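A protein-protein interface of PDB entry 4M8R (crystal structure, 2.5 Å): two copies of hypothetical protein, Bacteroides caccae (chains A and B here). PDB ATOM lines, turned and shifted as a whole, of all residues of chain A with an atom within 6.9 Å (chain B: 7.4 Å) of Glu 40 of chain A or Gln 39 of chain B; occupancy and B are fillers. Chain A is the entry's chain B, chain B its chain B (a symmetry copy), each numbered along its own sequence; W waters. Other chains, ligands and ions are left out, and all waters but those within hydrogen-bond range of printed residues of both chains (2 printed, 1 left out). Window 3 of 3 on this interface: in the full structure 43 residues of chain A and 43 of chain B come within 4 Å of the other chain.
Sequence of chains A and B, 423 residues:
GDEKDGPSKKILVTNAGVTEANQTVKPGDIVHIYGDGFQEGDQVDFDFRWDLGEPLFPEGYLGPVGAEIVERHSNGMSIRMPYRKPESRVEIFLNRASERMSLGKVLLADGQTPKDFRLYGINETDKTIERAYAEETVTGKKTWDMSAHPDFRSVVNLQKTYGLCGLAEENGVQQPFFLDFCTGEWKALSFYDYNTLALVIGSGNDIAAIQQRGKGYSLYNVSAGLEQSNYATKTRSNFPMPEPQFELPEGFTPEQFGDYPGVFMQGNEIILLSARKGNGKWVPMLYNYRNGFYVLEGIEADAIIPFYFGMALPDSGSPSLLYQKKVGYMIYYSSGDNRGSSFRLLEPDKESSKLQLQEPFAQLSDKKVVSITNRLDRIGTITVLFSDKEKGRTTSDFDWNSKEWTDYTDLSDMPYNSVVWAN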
ATOM      1  N   PHE A  38       5.217  25.628  10.852  1.00  0.00           N
ATOM      2  CA  PHE A  38       4.562  25.120  12.054  1.00  0.00           C
ATOM      3  C   PHE A  38       3.435  24.158  11.690  1.00  0.00           C
ATOM      4  O   PHE A  38       2.890  24.220  10.589  1.00  0.00           O
ATOM      5  CB  PHE A  38       4.027  26.258  12.909  1.00  0.00           C
ATOM      6  CG  PHE A  38       5.099  27.101  13.517  1.00  0.00           C
ATOM      7  CD1 PHE A  38       5.677  26.741  14.723  1.00  0.00           C
ATOM      8  CD2 PHE A  38       5.542  28.251  12.883  1.00  0.00           C
ATOM      9  CE1 PHE A  38       6.679  27.516  15.287  1.00  0.00           C
ATOM     10  CE2 PHE A  38       6.542  29.031  13.443  1.00  0.00           C
ATOM     11  CZ  PHE A  38       7.109  28.663  14.647  1.00  0.00           C
ATOM     12  N   GLN A  39       3.106  23.260  12.617  1.00  0.00           N
ATOM     13  CA  GLN A  39       2.133  22.199  12.364  1.00  0.00           C
ATOM     14  C   GLN A  39       1.182  22.041  13.535  1.00  0.00           C
ATOM     15  O   GLN A  39       1.520  22.383  14.671  1.00  0.00           O
ATOM     16  CB  GLN A  39       2.845  20.872  12.106  1.00  0.00           C
ATOM     17  CG  GLN A  39       3.830  20.917  10.948  1.00  0.00           C
ATOM     18  CD  GLN A  39       4.307  19.542  10.511  1.00  0.00           C
ATOM     19  OE1 GLN A  39       3.943  18.527  11.104  1.00  0.00           O
ATOM     20  NE2 GLN A  39       5.124  19.504   9.457  1.00  0.00           N
ATOM     21  N   GLU A  40      -0.018  21.538  13.248  1.00  0.00           N
ATOM     22  CA  GLU A  40      -0.994  21.243  14.297  1.00  0.00           C
ATOM     23  C   GLU A  40      -0.357  20.258  15.263  1.00  0.00           C
ATOM     24  O   GLU A  40       0.164  19.223  14.845  1.00  0.00           O
ATOM     25  CB  GLU A  40      -2.269  20.618  13.720  1.00  0.00           C
ATOM     26  CG  GLU A  40      -3.123  21.541  12.862  1.00  0.00           C
ATOM     27  CD  GLU A  40      -4.219  20.790  12.113  1.00  0.00           C
ATOM     28  OE1 GLU A  40      -4.848  19.885  12.712  1.00  0.00           O
ATOM     29  OE2 GLU A  40      -4.450  21.098  10.921  1.00  0.00           O
ATOM     30  N   GLY A  41      -0.395  20.579  16.544  1.00  0.00           N
ATOM     31  CA  GLY A  41       0.134  19.685  17.558  1.00  0.00           C
ATOM     32  C   GLY A  41       1.531  20.035  18.022  1.00  0.00           C
ATOM     33  O   GLY A  41       1.999  19.481  19.012  1.00  0.00           O
ATOM     34  N   ASP A  42       2.203  20.943  17.313  1.00  0.00           N
ATOM     35  CA  ASP A  42       3.481  21.460  17.780  1.00  0.00           C
ATOM     36  C   ASP A  42       3.300  22.031  19.181  1.00  0.00           C
ATOM     37  O   ASP A  42       2.323  22.723  19.452  1.00  0.00           O
ATOM     38  CB  ASP A  42       4.027  22.546  16.847  1.00  0.00           C
ATOM     39  CG  ASP A  42       4.638  21.983  15.569  1.00  0.00           C
ATOM     40  OD1 ASP A  42       4.516  20.767  15.323  1.00  0.00           O
ATOM     41  OD2 ASP A  42       5.240  22.766  14.797  1.00  0.00           O
ATOM     42  N   GLN A  43       4.234  21.713  20.070  1.00  0.00           N
ATOM     43  CA  GLN A  43       4.225  22.244  21.419  1.00  0.00           C
ATOM     44  C   GLN A  43       5.461  23.111  21.630  1.00  0.00           C
ATOM     45  O   GLN A  43       6.359  23.155  20.786  1.00  0.00           O
ATOM     46  CB  GLN A  43       4.143  21.105  22.434  1.00  0.00           C
ATOM     47  CG  GLN A  43       2.942  20.188  22.197  1.00  0.00           C
ATOM     48  CD  GLN A  43       2.602  19.282  23.375  1.00  0.00           C
ATOM     49  OE1 GLN A  43       3.022  19.517  24.511  1.00  0.00           O
ATOM     50  NE2 GLN A  43       1.829  18.232  23.104  1.00  0.00           N
ATOM     51  N   ARG A  72      -2.346  30.372  17.823  1.00  0.00           N
ATOM     52  CA  ARG A  72      -1.654  29.411  16.982  1.00  0.00           C
ATOM     53  C   ARG A  72      -1.999  29.615  15.503  1.00  0.00           C
ATOM     54  O   ARG A  72      -3.173  29.671  15.136  1.00  0.00           O
ATOM     55  CB  ARG A  72      -2.054  28.013  17.428  1.00  0.00           C
ATOM     56  CG  ARG A  72      -1.273  26.889  16.782  1.00  0.00           C
ATOM     57  CD  ARG A  72      -1.980  25.566  17.006  1.00  0.00           C
ATOM     58  NE  ARG A  72      -1.979  25.161  18.414  1.00  0.00           N
ATOM     59  CZ  ARG A  72      -1.001  24.479  19.012  1.00  0.00           C
ATOM     60  NH1 ARG A  72       0.098  24.112  18.343  1.00  0.00           N
ATOM     61  NH2 ARG A  72      -1.120  24.163  20.299  1.00  0.00           N
ATOM     62  N   ARG A  96       8.207  19.153  18.330  1.00  0.00           N
ATOM     63  CA  ARG A  96       7.391  18.389  17.390  1.00  0.00           C
ATOM     64  C   ARG A  96       7.593  16.894  17.634  1.00  0.00           C
ATOM     65  O   ARG A  96       8.533  16.295  17.112  1.00  0.00           O
ATOM     66  CB  ARG A  96       7.747  18.761  15.944  1.00  0.00           C
ATOM     67  CG  ARG A  96       7.004  17.954  14.882  1.00  0.00           C
ATOM     68  CD  ARG A  96       6.361  18.826  13.817  1.00  0.00           C
ATOM     69  NE  ARG A  96       7.305  19.328  12.822  1.00  0.00           N
ATOM     70  CZ  ARG A  96       7.478  20.608  12.480  1.00  0.00           C
ATOM     71  NH1 ARG A  96       6.777  21.590  13.039  1.00  0.00           N
ATOM     72  NH2 ARG A  96       8.374  20.907  11.558  1.00  0.00           N
ATOM     73  N   LEU B  12     -10.746  13.270  20.649  1.00  0.00           N
ATOM     74  CA  LEU B  12      -9.526  13.227  19.841  1.00  0.00           C
ATOM     75  C   LEU B  12      -9.509  12.060  18.859  1.00  0.00           C
ATOM     76  O   LEU B  12      -9.190  12.232  17.681  1.00  0.00           O
ATOM     77  CB  LEU B  12      -8.289  13.167  20.735  1.00  0.00           C
ATOM     78  CG  LEU B  12      -8.103  14.319  21.730  1.00  0.00           C
ATOM     79  CD1 LEU B  12      -6.771  14.174  22.454  1.00  0.00           C
ATOM     80  CD2 LEU B  12      -8.190  15.674  21.041  1.00  0.00           C
ATOM     81  N   VAL B  13      -9.857  10.875  19.350  1.00  0.00           N
ATOM     82  CA  VAL B  13      -9.842   9.663  18.538  1.00  0.00           C
ATOM     83  C   VAL B  13     -11.009   8.768  18.914  1.00  0.00           C
ATOM     84  O   VAL B  13     -11.436   8.730  20.071  1.00  0.00           O
ATOM     85  CB  VAL B  13      -8.514   8.875  18.691  1.00  0.00           C
ATOM     86  CG1 VAL B  13      -7.364   9.620  18.032  1.00  0.00           C
ATOM     87  CG2 VAL B  13      -8.190   8.598  20.155  1.00  0.00           C
ATOM     88  N   ASP B  36      -9.027   5.576  15.585  1.00  0.00           N
ATOM     89  CA  ASP B  36      -9.123   6.313  14.333  1.00  0.00           C
ATOM     90  C   ASP B  36      -8.975   7.803  14.616  1.00  0.00           C
ATOM     91  O   ASP B  36      -9.617   8.322  15.527  1.00  0.00           O
ATOM     92  CB  ASP B  36     -10.479   6.045  13.662  1.00  0.00           C
ATOM     93  CG  ASP B  36     -10.726   4.559  13.396  1.00  0.00           C
ATOM     94  OD1 ASP B  36      -9.760   3.831  13.079  1.00  0.00           O
ATOM     95  OD2 ASP B  36     -11.894   4.122  13.496  1.00  0.00           O
ATOM     96  N   GLY B  37      -8.131   8.483  13.843  1.00  0.00           N
ATOM     97  CA  GLY B  37      -8.003   9.939  13.926  1.00  0.00           C
ATOM     98  C   GLY B  37      -6.727  10.467  14.561  1.00  0.00           C
ATOM     99  O   GLY B  37      -6.659  11.642  14.922  1.00  0.00           O
ATOM    100  N   PHE B  38      -5.704   9.629  14.689  1.00  0.00           N
ATOM    101  CA  PHE B  38      -4.411  10.105  15.171  1.00  0.00           C
ATOM    102  C   PHE B  38      -3.796  11.092  14.183  1.00  0.00           C
ATOM    103  O   PHE B  38      -4.120  11.074  12.997  1.00  0.00           O
ATOM    104  CB  PHE B  38      -3.458   8.945  15.416  1.00  0.00           C
ATOM    105  CG  PHE B  38      -3.868   8.069  16.555  1.00  0.00           C
ATOM    106  CD1 PHE B  38      -3.495   8.381  17.852  1.00  0.00           C
ATOM    107  CD2 PHE B  38      -4.634   6.935  16.336  1.00  0.00           C
ATOM    108  CE1 PHE B  38      -3.881   7.575  18.912  1.00  0.00           C
ATOM    109  CE2 PHE B  38      -5.021   6.124  17.391  1.00  0.00           C
ATOM    110  CZ  PHE B  38      -4.642   6.444  18.680  1.00  0.00           C
ATOM    111  N   GLN B  39      -2.924  11.964  14.689  1.00  0.00           N
ATOM    112  CA  GLN B  39      -2.350  13.043  13.890  1.00  0.00           C
ATOM    113  C   GLN B  39      -0.859  13.175  14.139  1.00  0.00           C
ATOM    114  O   GLN B  39      -0.363  12.791  15.203  1.00  0.00           O
ATOM    115  CB  GLN B  39      -3.037  14.369  14.213  1.00  0.00           C
ATOM    116  CG  GLN B  39      -4.543  14.351  14.000  1.00  0.00           C
ATOM    117  CD  GLN B  39      -5.172  15.734  14.034  1.00  0.00           C
ATOM    118  OE1 GLN B  39      -4.493  16.734  14.271  1.00  0.00           O
ATOM    119  NE2 GLN B  39      -6.482  15.796  13.790  1.00  0.00           N
ATOM    120  N   GLU B  40      -0.146  13.703  13.146  1.00  0.00           N
ATOM    121  CA  GLU B  40       1.284  13.975  13.293  1.00  0.00           C
ATOM    122  C   GLU B  40       1.460  14.918  14.470  1.00  0.00           C
ATOM    123  O   GLU B  40       0.807  15.960  14.538  1.00  0.00           O
ATOM    124  CB  GLU B  40       1.864  14.634  12.037  1.00  0.00           C
ATOM    125  CG  GLU B  40       1.922  13.752  10.798  1.00  0.00           C
ATOM    126  CD  GLU B  40       2.255  14.542   9.537  1.00  0.00           C
ATOM    127  OE1 GLU B  40       3.135  15.434   9.598  1.00  0.00           O
ATOM    128  OE2 GLU B  40       1.634  14.276   8.482  1.00  0.00           O
ATOM    129  N   GLY B  41       2.335  14.556  15.393  1.00  0.00           N
ATOM    130  CA  GLY B  41       2.622  15.409  16.531  1.00  0.00           C
ATOM    131  C   GLY B  41       1.880  15.025  17.793  1.00  0.00           C
ATOM    132  O   GLY B  41       2.193  15.540  18.863  1.00  0.00           O
ATOM    133  N   ASP B  42       0.896  14.133  17.678  1.00  0.00           N
ATOM    134  CA  ASP B  42       0.243  13.584  18.858  1.00  0.00           C
ATOM    135  C   ASP B  42       1.300  12.969  19.767  1.00  0.00           C
ATOM    136  O   ASP B  42       2.202  12.280  19.297  1.00  0.00           O
ATOM    137  CB  ASP B  42      -0.799  12.523  18.486  1.00  0.00           C
ATOM    138  CG  ASP B  42      -2.096  13.121  17.955  1.00  0.00           C
ATOM    139  OD1 ASP B  42      -2.153  14.345  17.731  1.00  0.00           O
ATOM    140  OD2 ASP B  42      -3.068  12.356  17.750  1.00  0.00           O
ATOM    141  N   GLN B  43       1.195  13.245  21.061  1.00  0.00           N
ATOM    142  CA  GLN B  43       2.089  12.669  22.046  1.00  0.00           C
ATOM    143  C   GLN B  43       1.293  11.780  22.994  1.00  0.00           C
ATOM    144  O   GLN B  43       0.061  11.753  22.957  1.00  0.00           O
ATOM    145  CB  GLN B  43       2.838  13.775  22.789  1.00  0.00           C
ATOM    146  CG  GLN B  43       3.592  14.714  21.846  1.00  0.00           C
ATOM    147  CD  GLN B  43       4.639  15.585  22.531  1.00  0.00           C
ATOM    148  OE1 GLN B  43       5.075  15.307  23.651  1.00  0.00           O
ATOM    149  NE2 GLN B  43       5.051  16.652  21.851  1.00  0.00           N
ATOM    150  N   ARG B  72       4.519   4.751  14.727  1.00  0.00           N
ATOM    151  CA  ARG B  72       3.455   5.730  14.589  1.00  0.00           C
ATOM    152  C   ARG B  72       2.729   5.581  13.248  1.00  0.00           C
ATOM    153  O   ARG B  72       3.364   5.551  12.192  1.00  0.00           O
ATOM    154  CB  ARG B  72       4.068   7.118  14.705  1.00  0.00           C
ATOM    155  CG  ARG B  72       3.069   8.252  14.777  1.00  0.00           C
ATOM    156  CD  ARG B  72       3.764   9.576  14.520  1.00  0.00           C
ATOM    157  NE  ARG B  72       4.702   9.933  15.586  1.00  0.00           N
ATOM    158  CZ  ARG B  72       4.375  10.583  16.705  1.00  0.00           C
ATOM    159  NH1 ARG B  72       3.114  10.958  16.946  1.00  0.00           N
ATOM    160  NH2 ARG B  72       5.322  10.857  17.599  1.00  0.00           N
ATOM    161  N   HIS B  73       1.405   5.456  13.300  1.00  0.00           N
ATOM    162  CA  HIS B  73       0.565   5.513  12.098  1.00  0.00           C
ATOM    163  C   HIS B  73      -0.727   6.257  12.423  1.00  0.00           C
ATOM    164  O   HIS B  73      -0.909   6.742  13.534  1.00  0.00           O
ATOM    165  CB  HIS B  73       0.259   4.113  11.548  1.00  0.00           C
ATOM    166  CG  HIS B  73       1.355   3.125  11.773  1.00  0.00           C
ATOM    167  ND1 HIS B  73       1.429   2.378  12.923  1.00  0.00           N
ATOM    168  CD2 HIS B  73       2.425   2.771  11.020  1.00  0.00           C
ATOM    169  CE1 HIS B  73       2.496   1.601  12.872  1.00  0.00           C
ATOM    170  NE2 HIS B  73       3.118   1.818  11.728  1.00  0.00           N
ATOM    171  N   SER B  74      -1.616   6.348  11.441  1.00  0.00           N
ATOM    172  CA  SER B  74      -2.886   7.041  11.609  1.00  0.00           C
ATOM    173  C   SER B  74      -3.906   6.193  12.365  1.00  0.00           C
ATOM    174  O   SER B  74      -4.883   6.725  12.886  1.00  0.00           O
ATOM    175  CB  SER B  74      -3.451   7.433  10.244  1.00  0.00           C
ATOM    176  OG  SER B  74      -3.641   6.284   9.436  1.00  0.00           O
ATOM    177  N   MET B  77      -0.376   3.549  17.509  1.00  0.00           N
ATOM    178  CA  MET B  77       1.028   3.787  17.821  1.00  0.00           C
ATOM    179  C   MET B  77       1.548   2.779  18.810  1.00  0.00           C
ATOM    180  O   MET B  77       0.788   2.196  19.569  1.00  0.00           O
ATOM    181  CB  MET B  77       1.210   5.212  18.345  1.00  0.00           C
ATOM    182  CG  MET B  77       0.005   5.770  19.111  1.00  0.00           C
ATOM    183  SD  MET B  77      -0.036   7.725  18.968  1.00  0.00           S
ATOM    184  CE  MET B  77       1.888   8.089  19.151  1.00  0.00           C
ATOM    185  N   LEU B  94      -3.674  10.169  25.457  1.00  0.00           N
ATOM    186  CA  LEU B  94      -3.318  10.795  24.196  1.00  0.00           C
ATOM    187  C   LEU B  94      -3.263  12.300  24.420  1.00  0.00           C
ATOM    188  O   LEU B  94      -4.200  12.879  24.954  1.00  0.00           O
ATOM    189  CB  LEU B  94      -4.356  10.476  23.116  1.00  0.00           C
ATOM    190  CG  LEU B  94      -4.017  10.980  21.707  1.00  0.00           C
ATOM    191  CD1 LEU B  94      -2.739  10.328  21.195  1.00  0.00           C
ATOM    192  CD2 LEU B  94      -5.171  10.715  20.758  1.00  0.00           C
ATOM    193  N   ASN B  95      -2.171  12.925  23.999  1.00  0.00           N
ATOM    194  CA  ASN B  95      -1.965  14.359  24.190  1.00  0.00           C
ATOM    195  C   ASN B  95      -1.856  15.068  22.844  1.00  0.00           C
ATOM    196  O   ASN B  95      -0.849  14.931  22.147  1.00  0.00           O
ATOM    197  CB  ASN B  95      -0.699  14.584  25.024  1.00  0.00           C
ATOM    198  CG  ASN B  95      -0.440  16.053  25.337  1.00  0.00           C
ATOM    199  OD1 ASN B  95      -1.267  16.923  25.068  1.00  0.00           O
ATOM    200  ND2 ASN B  95       0.715  16.328  25.926  1.00  0.00           N
ATOM    201  N   ARG B  96      -2.900  15.811  22.480  1.00  0.00           N
ATOM    202  CA  ARG B  96      -2.903  16.617  21.262  1.00  0.00           C
ATOM    203  C   ARG B  96      -2.874  18.100  21.628  1.00  0.00           C
ATOM    204  O   ARG B  96      -3.915  18.703  21.882  1.00  0.00           O
ATOM    205  CB  ARG B  96      -4.133  16.288  20.404  1.00  0.00           C
ATOM    206  CG  ARG B  96      -4.272  17.141  19.145  1.00  0.00           C
ATOM    207  CD  ARG B  96      -4.508  16.313  17.893  1.00  0.00           C
ATOM    208  NE  ARG B  96      -5.880  15.832  17.758  1.00  0.00           N
ATOM    209  CZ  ARG B  96      -6.252  14.562  17.574  1.00  0.00           C
ATOM    210  NH1 ARG B  96      -5.370  13.571  17.495  1.00  0.00           N
ATOM    211  NH2 ARG B  96      -7.539  14.283  17.470  1.00  0.00           N
ATOM    212  N   ALA B  97      -1.669  18.672  21.664  1.00  0.00           N
ATOM    213  CA  ALA B  97      -1.453  20.065  22.081  1.00  0.00           C
ATOM    214  C   ALA B  97      -1.946  20.289  23.524  1.00  0.00           C
ATOM    215  O   ALA B  97      -1.415  19.694  24.462  1.00  0.00           O
ATOM    216  CB  ALA B  97      -2.111  21.026  21.090  1.00  0.00           C
HETATM  217  O   HOH W   1       1.335  19.218  27.021  1.00  0.00           O
HETATM  218  O   HOH W   2       4.197  17.539  19.062  1.00  0.00           O
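Of the 8 printed residues of chain A, 5 touch a printed residue of chain B. Printed residues of chain A that touch a printed residue of chain B: Gln 39, Glu 40, Gly 41, Gln 43 and Arg 72. Of the 18 printed residues of chain B, 6 touch a printed residue of chain A. Printed residues of chain B that touch a printed residue of chain A: Gln 39, Glu 40, Gly 41, Gln 43, Asn 95 and Ala 97. Hydrophobic or aromatic side chains of chain B that line the printed part of chain A: Ala 97. Among the printed residues, 8 pairs touch across the chains. Among the printed residues, no Asp or Glu carboxylate lies within 4 Å of a Lys or Arg side-chain nitrogen of the other chain.
Among the printed residues, pairs that only touch across the chains: Gln 39 of chain A with Glu 40 of chain B (3.5 Å), Glu 40 of chain A with Gln 39 of chain B (3.5 Å), Gly 41 of chain A with Gly 41 of chain B (3.9 Å), Gln 43 of chain A with Gln 43 of chain B (3.8 Å), Gln 43 of chain A with Asn 95 of chain B (3.6 Å), Gln 43 of chain A with Ala 97 of chain B (3.8 Å) and Arg 72 of chain A with Ala 97 of chain B (3.4 Å).
The backbone carbonyl oxygen of Glu 40 of chain B sits close to the backbone carbonyl oxygen of Glu 40 of chain A (3.3 Å).
Water W2 lies within hydrogen-bond range of O of Gly 41 of chain B (2.8 Å), O of Gly 41 of chain A (2.9 Å) and NE2 of Gln 43 of chain B (3.0 Å). Water W1 lies within hydrogen-bond range of the side-chain amide oxygen of Gln 43 of chain A and the side-chain amide nitrogen of Asn 95 of chain B.
Of chain B, only Gln 39 (3.5 Å) and Glu 40 (3.3 Å) come within 4 Å of Glu 40 of chain A. Of the printed residues of chain B, Arg 72 of chain A touches Ala 97 (3.4 Å). Of the printed residues of chain A, Gln 43 of chain B touches Gln 43 (3.8 Å). His 73 of chain B touches none of the printed residues of chain A. Of the printed residues of chain A, Asn 95 of chain B touches Gln 43. Printed residues of chain A within 4 Å of Ala 97 of chain B: Gln 43 and Arg 72. The nearest residue of chain B that does not touch Glu 40 of chain A is Gly 41 of chain B (4.8 Å). The nearest printed residue of chain A that does not touch Glu 40 of chain B is Gly 41 of chain A (4.8 Å).
N of Gln 39 of chain A lies within hydrogen-bond range of OD2 of Asp 42 of chain A (3.1 Å). N of Asn 95 of chain B is in hydrogen-bond range of O of Gln 43 of chain B, 2.7 Å away. OD1 of Asn 95 of chain B lies close to O of Ala 97 of chain B (2.8 Å). The guanidinium group (NH1) of Arg 72 of chain A sits at hydrogen-bond distance from the backbone carbonyl oxygen (O) of Asp 42 of chain A (2.8 Å). The side-chain carboxylate (OD2) of Asp 42 of chain B lies within hydrogen-bond range of the backbone NH (N) of Gln 39 of chain B (3.1 Å).
Gln 39 of chain A touches Glu 40 of chain B, and with the chains exchanged Glu 40 of chain A touches Gln 39 of chain B. Glu 40 of chain A touches its own counterpart, Glu 40 of chain B. Gly 41 of chain B touches its own counterpart, Gly 41 of chain A. Gln 43 of chain B touches its own counterpart, Gln 43 of chain A. Positions printed for both chains: 38, 39, 40, 41, 42, 43, 72 and 96. Of the 8 pairs that touch across the chains among the printed residues, 5 have their exchanged pair printed and touching as well.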
